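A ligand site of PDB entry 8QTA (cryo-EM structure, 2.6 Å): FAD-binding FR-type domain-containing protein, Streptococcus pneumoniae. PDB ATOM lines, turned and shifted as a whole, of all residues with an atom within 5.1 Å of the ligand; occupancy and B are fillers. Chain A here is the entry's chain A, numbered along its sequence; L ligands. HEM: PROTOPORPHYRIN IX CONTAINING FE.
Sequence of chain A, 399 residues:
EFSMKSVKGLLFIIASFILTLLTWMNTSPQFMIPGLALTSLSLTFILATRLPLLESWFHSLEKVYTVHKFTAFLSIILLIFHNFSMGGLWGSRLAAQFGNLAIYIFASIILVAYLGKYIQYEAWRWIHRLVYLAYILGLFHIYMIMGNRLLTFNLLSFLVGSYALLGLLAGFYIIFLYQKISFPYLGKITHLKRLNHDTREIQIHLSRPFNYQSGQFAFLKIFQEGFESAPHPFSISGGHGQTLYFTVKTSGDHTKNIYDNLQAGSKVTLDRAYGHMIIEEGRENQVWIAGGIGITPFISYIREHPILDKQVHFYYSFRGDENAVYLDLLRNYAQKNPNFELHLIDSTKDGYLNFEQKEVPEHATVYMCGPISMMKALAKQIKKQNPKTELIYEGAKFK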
ATOM      1  N   TRP A  24      25.426  -2.374  21.755  1.00  0.00           N
ATOM      2  CA  TRP A  24      24.393  -1.873  22.660  1.00  0.00           C
ATOM      3  C   TRP A  24      23.300  -2.911  22.880  1.00  0.00           C
ATOM      4  O   TRP A  24      22.848  -3.103  24.017  1.00  0.00           O
ATOM      5  CB  TRP A  24      23.800  -0.579  22.111  1.00  0.00           C
ATOM      6  CG  TRP A  24      24.615   0.617  22.452  1.00  0.00           C
ATOM      7  CD1 TRP A  24      25.397   1.340  21.605  1.00  0.00           C
ATOM      8  CD2 TRP A  24      24.748   1.227  23.743  1.00  0.00           C
ATOM      9  NE1 TRP A  24      26.009   2.365  22.288  1.00  0.00           N
ATOM     10  CE2 TRP A  24      25.628   2.314  23.597  1.00  0.00           C
ATOM     11  CE3 TRP A  24      24.204   0.954  25.001  1.00  0.00           C
ATOM     12  CZ2 TRP A  24      25.968   3.140  24.668  1.00  0.00           C
ATOM     13  CZ3 TRP A  24      24.546   1.773  26.061  1.00  0.00           C
ATOM     14  CH2 TRP A  24      25.421   2.848  25.887  1.00  0.00           C
ATOM     15  N   PHE A  31      19.218   1.521  25.270  1.00  0.00           N
ATOM     16  CA  PHE A  31      20.011   2.672  24.839  1.00  0.00           C
ATOM     17  C   PHE A  31      20.601   2.475  23.456  1.00  0.00           C
ATOM     18  O   PHE A  31      21.661   3.026  23.155  1.00  0.00           O
ATOM     19  CB  PHE A  31      21.130   2.956  25.836  1.00  0.00           C
ATOM     20  CG  PHE A  31      20.644   3.393  27.189  1.00  0.00           C
ATOM     21  CD1 PHE A  31      19.674   4.367  27.320  1.00  0.00           C
ATOM     22  CD2 PHE A  31      21.174   2.823  28.342  1.00  0.00           C
ATOM     23  CE1 PHE A  31      19.242   4.768  28.572  1.00  0.00           C
ATOM     24  CE2 PHE A  31      20.744   3.216  29.583  1.00  0.00           C
ATOM     25  CZ  PHE A  31      19.777   4.183  29.701  1.00  0.00           C
ATOM     26  N   PRO A  34      20.010   6.292  21.566  1.00  0.00           N
ATOM     27  CA  PRO A  34      21.028   7.259  22.010  1.00  0.00           C
ATOM     28  C   PRO A  34      22.442   6.797  21.755  1.00  0.00           C
ATOM     29  O   PRO A  34      23.320   7.636  21.495  1.00  0.00           O
ATOM     30  CB  PRO A  34      20.734   7.413  23.512  1.00  0.00           C
ATOM     31  CG  PRO A  34      19.979   6.212  23.888  1.00  0.00           C
ATOM     32  CD  PRO A  34      19.151   5.879  22.691  1.00  0.00           C
ATOM     33  N   GLY A  35      22.713   5.497  21.835  1.00  0.00           N
ATOM     34  CA  GLY A  35      24.043   4.999  21.553  1.00  0.00           C
ATOM     35  C   GLY A  35      24.414   5.144  20.082  1.00  0.00           C
ATOM     36  O   GLY A  35      25.564   5.452  19.756  1.00  0.00           O
ATOM     37  N   LEU A  38      25.366   8.839  19.252  1.00  0.00           N
ATOM     38  CA  LEU A  38      26.711   9.228  19.666  1.00  0.00           C
ATOM     39  C   LEU A  38      27.765   8.764  18.670  1.00  0.00           C
ATOM     40  O   LEU A  38      28.764   9.463  18.455  1.00  0.00           O
ATOM     41  CB  LEU A  38      27.002   8.665  21.069  1.00  0.00           C
ATOM     42  CG  LEU A  38      28.462   8.651  21.530  1.00  0.00           C
ATOM     43  CD1 LEU A  38      28.960  10.062  21.781  1.00  0.00           C
ATOM     44  CD2 LEU A  38      28.607   7.802  22.783  1.00  0.00           C
ATOM     45  N   LEU A  41      27.504  11.206  15.824  1.00  0.00           N
ATOM     46  CA  LEU A  41      28.137  12.458  16.207  1.00  0.00           C
ATOM     47  C   LEU A  41      29.653  12.347  16.148  1.00  0.00           C
ATOM     48  O   LEU A  41      30.342  13.309  15.783  1.00  0.00           O
ATOM     49  CB  LEU A  41      27.696  12.866  17.611  1.00  0.00           C
ATOM     50  CG  LEU A  41      26.265  13.407  17.751  1.00  0.00           C
ATOM     51  CD1 LEU A  41      25.885  13.495  19.218  1.00  0.00           C
ATOM     52  CD2 LEU A  41      26.140  14.759  17.080  1.00  0.00           C
ATOM     53  N   LEU A  79      18.559  11.802  18.386  1.00  0.00           N
ATOM     54  CA  LEU A  79      18.557  12.514  19.661  1.00  0.00           C
ATOM     55  C   LEU A  79      17.190  13.100  19.977  1.00  0.00           C
ATOM     56  O   LEU A  79      16.823  13.205  21.147  1.00  0.00           O
ATOM     57  CB  LEU A  79      19.615  13.619  19.643  1.00  0.00           C
ATOM     58  CG  LEU A  79      21.069  13.174  19.592  1.00  0.00           C
ATOM     59  CD1 LEU A  79      22.001  14.379  19.560  1.00  0.00           C
ATOM     60  CD2 LEU A  79      21.386  12.280  20.769  1.00  0.00           C
ATOM     61  N   HIS A  82      15.335  10.282  21.195  1.00  0.00           N
ATOM     62  CA  HIS A  82      15.846  10.023  22.536  1.00  0.00           C
ATOM     63  C   HIS A  82      15.214  10.978  23.548  1.00  0.00           C
ATOM     64  O   HIS A  82      14.742  10.551  24.602  1.00  0.00           O
ATOM     65  CB  HIS A  82      17.363  10.160  22.557  1.00  0.00           C
ATOM     66  CG  HIS A  82      17.976   9.898  23.910  1.00  0.00           C
ATOM     67  ND1 HIS A  82      17.581   8.849  24.709  1.00  0.00           N
ATOM     68  CD2 HIS A  82      18.945  10.555  24.590  1.00  0.00           C
ATOM     69  CE1 HIS A  82      18.292   8.871  25.824  1.00  0.00           C
ATOM     70  NE2 HIS A  82      19.123   9.892  25.773  1.00  0.00           N
ATOM     71  N   ASN A  83      15.187  12.265  23.229  1.00  0.00           N
ATOM     72  CA  ASN A  83      14.600  13.249  24.134  1.00  0.00           C
ATOM     73  C   ASN A  83      13.103  13.043  24.296  1.00  0.00           C
ATOM     74  O   ASN A  83      12.567  13.163  25.404  1.00  0.00           O
ATOM     75  CB  ASN A  83      14.895  14.661  23.619  1.00  0.00           C
ATOM     76  CG  ASN A  83      14.195  15.739  24.424  1.00  0.00           C
ATOM     77  OD1 ASN A  83      13.953  15.574  25.617  1.00  0.00           O
ATOM     78  ND2 ASN A  83      13.882  16.849  23.776  1.00  0.00           N
ATOM     79  N   MET A  86      12.353   9.840  26.507  1.00  0.00           N
ATOM     80  CA  MET A  86      13.083   9.697  27.746  1.00  0.00           C
ATOM     81  C   MET A  86      13.030  10.911  28.664  1.00  0.00           C
ATOM     82  O   MET A  86      13.429  10.792  29.821  1.00  0.00           O
ATOM     83  CB  MET A  86      14.549   9.347  27.453  1.00  0.00           C
ATOM     84  CG  MET A  86      15.274   8.624  28.563  1.00  0.00           C
ATOM     85  SD  MET A  86      14.977   6.848  28.486  1.00  0.00           S
ATOM     86  CE  MET A  86      16.367   6.320  27.496  1.00  0.00           C
ATOM     87  N   GLY A  87      12.554  12.044  28.196  1.00  0.00           N
ATOM     88  CA  GLY A  87      12.492  13.236  29.017  1.00  0.00           C
ATOM     89  C   GLY A  87      11.572  14.288  28.467  1.00  0.00           C
ATOM     90  O   GLY A  87      10.591  13.987  27.794  1.00  0.00           O
ATOM     91  N   GLY A  88      11.892  15.552  28.770  1.00  0.00           N
ATOM     92  CA  GLY A  88      11.058  16.667  28.363  1.00  0.00           C
ATOM     93  C   GLY A  88      11.865  17.874  27.920  1.00  0.00           C
ATOM     94  O   GLY A  88      12.945  17.732  27.337  1.00  0.00           O
ATOM     95  N   LEU A  89      11.334  19.074  28.172  1.00  0.00           N
ATOM     96  CA  LEU A  89      12.012  20.288  27.742  1.00  0.00           C
ATOM     97  C   LEU A  89      13.234  20.583  28.602  1.00  0.00           C
ATOM     98  O   LEU A  89      14.286  20.972  28.080  1.00  0.00           O
ATOM     99  CB  LEU A  89      11.045  21.462  27.765  1.00  0.00           C
ATOM    100  CG  LEU A  89       9.823  21.382  26.856  1.00  0.00           C
ATOM    101  CD1 LEU A  89       8.978  22.638  26.986  1.00  0.00           C
ATOM    102  CD2 LEU A  89      10.234  21.156  25.415  1.00  0.00           C
ATOM    103  N   TRP A  90      13.117  20.422  29.914  1.00  0.00           N
ATOM    104  CA  TRP A  90      14.212  20.690  30.833  1.00  0.00           C
ATOM    105  C   TRP A  90      14.293  19.573  31.848  1.00  0.00           C
ATOM    106  O   TRP A  90      13.284  18.988  32.243  1.00  0.00           O
ATOM    107  CB  TRP A  90      14.037  22.056  31.533  1.00  0.00           C
ATOM    108  CG  TRP A  90      15.287  22.600  32.155  1.00  0.00           C
ATOM    109  CD1 TRP A  90      15.463  22.948  33.465  1.00  0.00           C
ATOM    110  CD2 TRP A  90      16.534  22.864  31.500  1.00  0.00           C
ATOM    111  NE1 TRP A  90      16.746  23.410  33.661  1.00  0.00           N
ATOM    112  CE2 TRP A  90      17.415  23.368  32.467  1.00  0.00           C
ATOM    113  CE3 TRP A  90      16.988  22.722  30.185  1.00  0.00           C
ATOM    114  CZ2 TRP A  90      18.726  23.728  32.166  1.00  0.00           C
ATOM    115  CZ3 TRP A  90      18.287  23.091  29.892  1.00  0.00           C
ATOM    116  CH2 TRP A  90      19.139  23.581  30.879  1.00  0.00           C
ATOM    117  N   GLY A  91      15.517  19.264  32.281  1.00  0.00           N
ATOM    118  CA  GLY A  91      15.742  18.144  33.158  1.00  0.00           C
ATOM    119  C   GLY A  91      15.728  18.513  34.628  1.00  0.00           C
ATOM    120  O   GLY A  91      15.858  19.664  35.011  1.00  0.00           O
ATOM    121  N   SER A  92      15.559  17.484  35.465  1.00  0.00           N
ATOM    122  CA  SER A  92      15.515  17.652  36.913  1.00  0.00           C
ATOM    123  C   SER A  92      16.902  17.570  37.550  1.00  0.00           C
ATOM    124  O   SER A  92      17.196  18.329  38.479  1.00  0.00           O
ATOM    125  CB  SER A  92      14.591  16.611  37.538  1.00  0.00           C
ATOM    126  OG  SER A  92      14.859  16.468  38.917  1.00  0.00           O
ATOM    127  N   ARG A  93      17.751  16.672  37.073  1.00  0.00           N
ATOM    128  CA  ARG A  93      19.108  16.552  37.569  1.00  0.00           C
ATOM    129  C   ARG A  93      20.071  17.299  36.659  1.00  0.00           C
ATOM    130  O   ARG A  93      19.739  17.674  35.539  1.00  0.00           O
ATOM    131  CB  ARG A  93      19.518  15.073  37.679  1.00  0.00           C
ATOM    132  CG  ARG A  93      18.406  14.125  38.059  1.00  0.00           C
ATOM    133  CD  ARG A  93      18.674  12.728  37.534  1.00  0.00           C
ATOM    134  NE  ARG A  93      20.058  12.313  37.784  1.00  0.00           N
ATOM    135  CZ  ARG A  93      20.642  11.285  37.194  1.00  0.00           C
ATOM    136  NH1 ARG A  93      19.998  10.534  36.313  1.00  0.00           N
ATOM    137  NH2 ARG A  93      21.905  10.990  37.501  1.00  0.00           N
ATOM    138  N   ALA A  96      20.827  15.183  33.439  1.00  0.00           N
ATOM    139  CA  ALA A  96      19.819  15.296  32.381  1.00  0.00           C
ATOM    140  C   ALA A  96      19.865  16.655  31.704  1.00  0.00           C
ATOM    141  O   ALA A  96      19.679  16.751  30.491  1.00  0.00           O
ATOM    142  CB  ALA A  96      18.433  15.024  32.966  1.00  0.00           C
ATOM    143  N   GLY A  99      22.215  17.036  28.801  1.00  0.00           N
ATOM    144  CA  GLY A  99      21.679  16.571  27.534  1.00  0.00           C
ATOM    145  C   GLY A  99      20.627  17.496  26.959  1.00  0.00           C
ATOM    146  O   GLY A  99      20.416  17.502  25.735  1.00  0.00           O
ATOM    147  N   ASN A 100      19.967  18.274  27.804  1.00  0.00           N
ATOM    148  CA  ASN A 100      19.043  19.295  27.320  1.00  0.00           C
ATOM    149  C   ASN A 100      19.791  20.426  26.628  1.00  0.00           C
ATOM    150  O   ASN A 100      19.411  20.861  25.532  1.00  0.00           O
ATOM    151  CB  ASN A 100      18.201  19.838  28.474  1.00  0.00           C
ATOM    152  CG  ASN A 100      16.958  19.014  28.726  1.00  0.00           C
ATOM    153  OD1 ASN A 100      16.700  18.607  29.857  1.00  0.00           O
ATOM    154  ND2 ASN A 100      16.188  18.776  27.683  1.00  0.00           N
ATOM    155  N   ALA A 102      22.782  20.304  25.272  1.00  0.00           N
ATOM    156  CA  ALA A 102      23.437  19.814  24.069  1.00  0.00           C
ATOM    157  C   ALA A 102      22.473  19.706  22.900  1.00  0.00           C
ATOM    158  O   ALA A 102      22.798  20.085  21.773  1.00  0.00           O
ATOM    159  CB  ALA A 102      24.111  18.472  24.338  1.00  0.00           C
ATOM    160  N   ILE A 103      21.265  19.194  23.151  1.00  0.00           N
ATOM    161  CA  ILE A 103      20.300  19.039  22.067  1.00  0.00           C
ATOM    162  C   ILE A 103      19.797  20.391  21.575  1.00  0.00           C
ATOM    163  O   ILE A 103      19.464  20.543  20.394  1.00  0.00           O
ATOM    164  CB  ILE A 103      19.150  18.113  22.484  1.00  0.00           C
ATOM    165  CG1 ILE A 103      18.495  17.494  21.244  1.00  0.00           C
ATOM    166  CG2 ILE A 103      18.118  18.847  23.312  1.00  0.00           C
ATOM    167  CD1 ILE A 103      17.485  16.420  21.559  1.00  0.00           C
ATOM    168  N   PHE A 106      22.690  21.582  19.426  1.00  0.00           N
ATOM    169  CA  PHE A 106      22.778  20.756  18.224  1.00  0.00           C
ATOM    170  C   PHE A 106      21.693  21.122  17.222  1.00  0.00           C
ATOM    171  O   PHE A 106      21.944  21.205  16.021  1.00  0.00           O
ATOM    172  CB  PHE A 106      22.691  19.275  18.593  1.00  0.00           C
ATOM    173  CG  PHE A 106      24.020  18.656  18.909  1.00  0.00           C
ATOM    174  CD1 PHE A 106      25.101  18.833  18.076  1.00  0.00           C
ATOM    175  CD2 PHE A 106      24.181  17.883  20.046  1.00  0.00           C
ATOM    176  CE1 PHE A 106      26.319  18.263  18.369  1.00  0.00           C
ATOM    177  CE2 PHE A 106      25.394  17.301  20.345  1.00  0.00           C
ATOM    178  CZ  PHE A 106      26.469  17.491  19.503  1.00  0.00           C
ATOM    179  N   GLY A 138      27.307  16.802  25.772  1.00  0.00           N
ATOM    180  CA  GLY A 138      26.734  15.475  25.650  1.00  0.00           C
ATOM    181  C   GLY A 138      27.595  14.402  26.284  1.00  0.00           C
ATOM    182  O   GLY A 138      27.074  13.431  26.834  1.00  0.00           O
ATOM    183  N   HIS A 141      26.878  14.387  29.800  1.00  0.00           N
ATOM    184  CA  HIS A 141      25.577  13.769  30.013  1.00  0.00           C
ATOM    185  C   HIS A 141      25.675  12.250  30.008  1.00  0.00           C
ATOM    186  O   HIS A 141      25.075  11.577  30.842  1.00  0.00           O
ATOM    187  CB  HIS A 141      24.596  14.251  28.946  1.00  0.00           C
ATOM    188  CG  HIS A 141      23.346  13.447  28.863  1.00  0.00           C
ATOM    189  ND1 HIS A 141      22.314  13.554  29.780  1.00  0.00           N
ATOM    190  CD2 HIS A 141      22.937  12.510  27.966  1.00  0.00           C
ATOM    191  CE1 HIS A 141      21.342  12.728  29.445  1.00  0.00           C
ATOM    192  NE2 HIS A 141      21.696  12.086  28.351  1.00  0.00           N
ATOM    193  N   ILE A 142      26.445  11.691  29.064  1.00  0.00           N
ATOM    194  CA  ILE A 142      26.544  10.238  28.946  1.00  0.00           C
ATOM    195  C   ILE A 142      27.293   9.656  30.136  1.00  0.00           C
ATOM    196  O   ILE A 142      26.884   8.636  30.710  1.00  0.00           O
ATOM    197  CB  ILE A 142      27.232   9.856  27.621  1.00  0.00           C
ATOM    198  CG1 ILE A 142      26.388  10.330  26.435  1.00  0.00           C
ATOM    199  CG2 ILE A 142      27.450   8.368  27.545  1.00  0.00           C
ATOM    200  CD1 ILE A 142      27.132  10.347  25.129  1.00  0.00           C
ATOM    201  N   ILE A 145      25.350  10.014  33.488  1.00  0.00           N
ATOM    202  CA  ILE A 145      24.202   9.116  33.543  1.00  0.00           C
ATOM    203  C   ILE A 145      24.652   7.676  33.721  1.00  0.00           C
ATOM    204  O   ILE A 145      24.232   6.987  34.655  1.00  0.00           O
ATOM    205  CB  ILE A 145      23.333   9.278  32.285  1.00  0.00           C
ATOM    206  CG1 ILE A 145      22.515  10.574  32.347  1.00  0.00           C
ATOM    207  CG2 ILE A 145      22.430   8.081  32.110  1.00  0.00           C
ATOM    208  CD1 ILE A 145      21.308  10.504  33.244  1.00  0.00           C
ATOM    209  N   MET A 146      25.520   7.209  32.825  1.00  0.00           N
ATOM    210  CA  MET A 146      26.001   5.822  32.853  1.00  0.00           C
ATOM    211  C   MET A 146      27.360   5.753  33.560  1.00  0.00           C
ATOM    212  O   MET A 146      28.376   5.385  32.980  1.00  0.00           O
ATOM    213  CB  MET A 146      26.081   5.262  31.439  1.00  0.00           C
ATOM    214  CG  MET A 146      24.735   5.091  30.757  1.00  0.00           C
ATOM    215  SD  MET A 146      24.246   3.366  30.608  1.00  0.00           S
ATOM    216  CE  MET A 146      25.636   2.694  29.709  1.00  0.00           C
HETATM  217  CHA HEM L   1      17.859  11.733  28.672  1.00  0.00           C
HETATM  218  CHB HEM L   1      21.087   8.124  28.546  1.00  0.00           C
HETATM  219  CHC HEM L   1      23.026  10.196  24.632  1.00  0.00           C
HETATM  220  CHD HEM L   1      20.188  14.026  25.157  1.00  0.00           C
HETATM  221  C1A HEM L   1      18.575  10.609  28.971  1.00  0.00           C
HETATM  222  C2A HEM L   1      18.283   9.750  30.010  1.00  0.00           C
HETATM  223  C3A HEM L   1      19.172   8.738  29.994  1.00  0.00           C
HETATM  224  C4A HEM L   1      20.040   8.944  28.924  1.00  0.00           C
HETATM  225  CMA HEM L   1      19.188   7.600  30.960  1.00  0.00           C
HETATM  226  CAA HEM L   1      17.165   9.907  30.998  1.00  0.00           C
HETATM  227  CBA HEM L   1      17.286  11.250  31.682  1.00  0.00           C
HETATM  228  CGA HEM L   1      16.968  11.102  33.115  1.00  0.00           C
HETATM  229  O1A HEM L   1      15.911  11.584  33.539  1.00  0.00           O
HETATM  230  O2A HEM L   1      17.767  10.532  33.879  1.00  0.00           O
HETATM  231  C1B HEM L   1      21.858   8.373  27.401  1.00  0.00           C
HETATM  232  C2B HEM L   1      22.841   7.479  26.904  1.00  0.00           C
HETATM  233  C3B HEM L   1      23.393   8.058  25.810  1.00  0.00           C
HETATM  234  C4B HEM L   1      22.708   9.335  25.651  1.00  0.00           C
HETATM  235  CMB HEM L   1      23.213   6.148  27.500  1.00  0.00           C
HETATM  236  CAB HEM L   1      24.447   7.672  24.867  1.00  0.00           C
HETATM  237  CBB HEM L   1      25.142   6.548  24.865  1.00  0.00           C
HETATM  238  C1C HEM L   1      22.547  11.489  24.535  1.00  0.00           C
HETATM  239  C2C HEM L   1      23.131  12.556  23.859  1.00  0.00           C
HETATM  240  C3C HEM L   1      22.283  13.640  24.039  1.00  0.00           C
HETATM  241  C4C HEM L   1      21.225  13.214  24.821  1.00  0.00           C
HETATM  242  CMC HEM L   1      24.432  12.436  23.105  1.00  0.00           C
HETATM  243  CAC HEM L   1      22.303  15.045  23.594  1.00  0.00           C
HETATM  244  CBC HEM L   1      23.096  15.511  22.658  1.00  0.00           C
HETATM  245  C1D HEM L   1      19.292  13.640  26.135  1.00  0.00           C
HETATM  246  C2D HEM L   1      18.159  14.466  26.486  1.00  0.00           C
HETATM  247  C3D HEM L   1      17.529  13.839  27.454  1.00  0.00           C
HETATM  248  C4D HEM L   1      18.261  12.621  27.711  1.00  0.00           C
HETATM  249  CMD HEM L   1      17.779  15.773  25.903  1.00  0.00           C
HETATM  250  CAD HEM L   1      16.311  14.344  28.124  1.00  0.00           C
HETATM  251  CBD HEM L   1      16.780  14.953  29.419  1.00  0.00           C
HETATM  252  CGD HEM L   1      15.590  15.138  30.271  1.00  0.00           C
HETATM  253  O1D HEM L   1      15.613  14.837  31.449  1.00  0.00           O
HETATM  254  O2D HEM L   1      14.549  15.570  29.826  1.00  0.00           O
HETATM  255  NA  HEM L   1      19.671  10.117  28.329  1.00  0.00           N
HETATM  256  NB  HEM L   1      21.812   9.458  26.617  1.00  0.00           N
HETATM  257  NC  HEM L   1      21.431  11.913  25.130  1.00  0.00           N
HETATM  258  ND  HEM L   1      19.312  12.543  26.896  1.00  0.00           N
HETATM  259 FE   HEM L   1      20.529  11.107  26.829  1.00  0.00          FE
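A ring nitrogen (NE2) of His 82 binds an iron atom (FE) of the ligand (2.1 Å).
FE of the ligand is bound by NE2 of His 141 (2.2 Å).
The backbone NH (N) of Gly 88 is in hydrogen-bond range of an oxygen (O2D) of the ligand (2.9 Å).
The guanidinium group (NH1) of Arg 93 lies within salt-bridge range of an oxygen (O2A) of the ligand (3.3 Å).
Trp 24 touches the ligand (CZ2 to CBB, 3.5 Å).
Phe 31 touches the ligand (CZ to CMA, 3.7 Å).
CB of Pro 34 touches C4B of the ligand (3.5 Å).
Gly 35 touches the ligand (CA to CBB, 3.8 Å).
Leu 79 touches the ligand (CD1 to CBC, 3.5 Å).
Asn 83 touches the ligand.
Met 86 touches the ligand.
Gly 87 touches the ligand (CA to O2D, 3.2 Å).
CA of Gly 91 touches O1D of the ligand, at 3.7 Å.
Ala 96 touches the ligand (CB to O1D, 3.2 Å).
Gly 99 touches the ligand (O to CMD, 3.2 Å).
Asn 100 touches the ligand.
Ala 102 touches the ligand (CB to CBC, 3.6 Å).
CD2 of Phe 106 touches CBC of the ligand, at 3.7 Å.
Ile 142 touches the ligand.
CG2 of Ile 145 touches CMA of the ligand, 3.5 Å away.
Met 146 touches the ligand.
Hydrophobic or aromatic side chains that line the ligand: Trp 24, Phe 31, Pro 34, Leu 79, His 82, Met 86, Ala 96, Ala 102, Phe 106, His 141, Ile 142, Ile 145 and Met 146.
Along chain A the residues within 4 Å of the ligand span positions 24 to 146.
O of Gly 88 sits close to OD1 of Asn 83 (2.9 Å).
The backbone carbonyl oxygen of Gly 88 lies within hydrogen-bond range of the side-chain amide nitrogen of Asn 100 (3.4 Å).
N of Gly 91 sits at hydrogen-bond distance from OD1 of Asn 100 (2.8 Å).
The side-chain amide nitrogen of Asn 100 lies within hydrogen-bond range of the backbone carbonyl oxygen of Leu 89.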
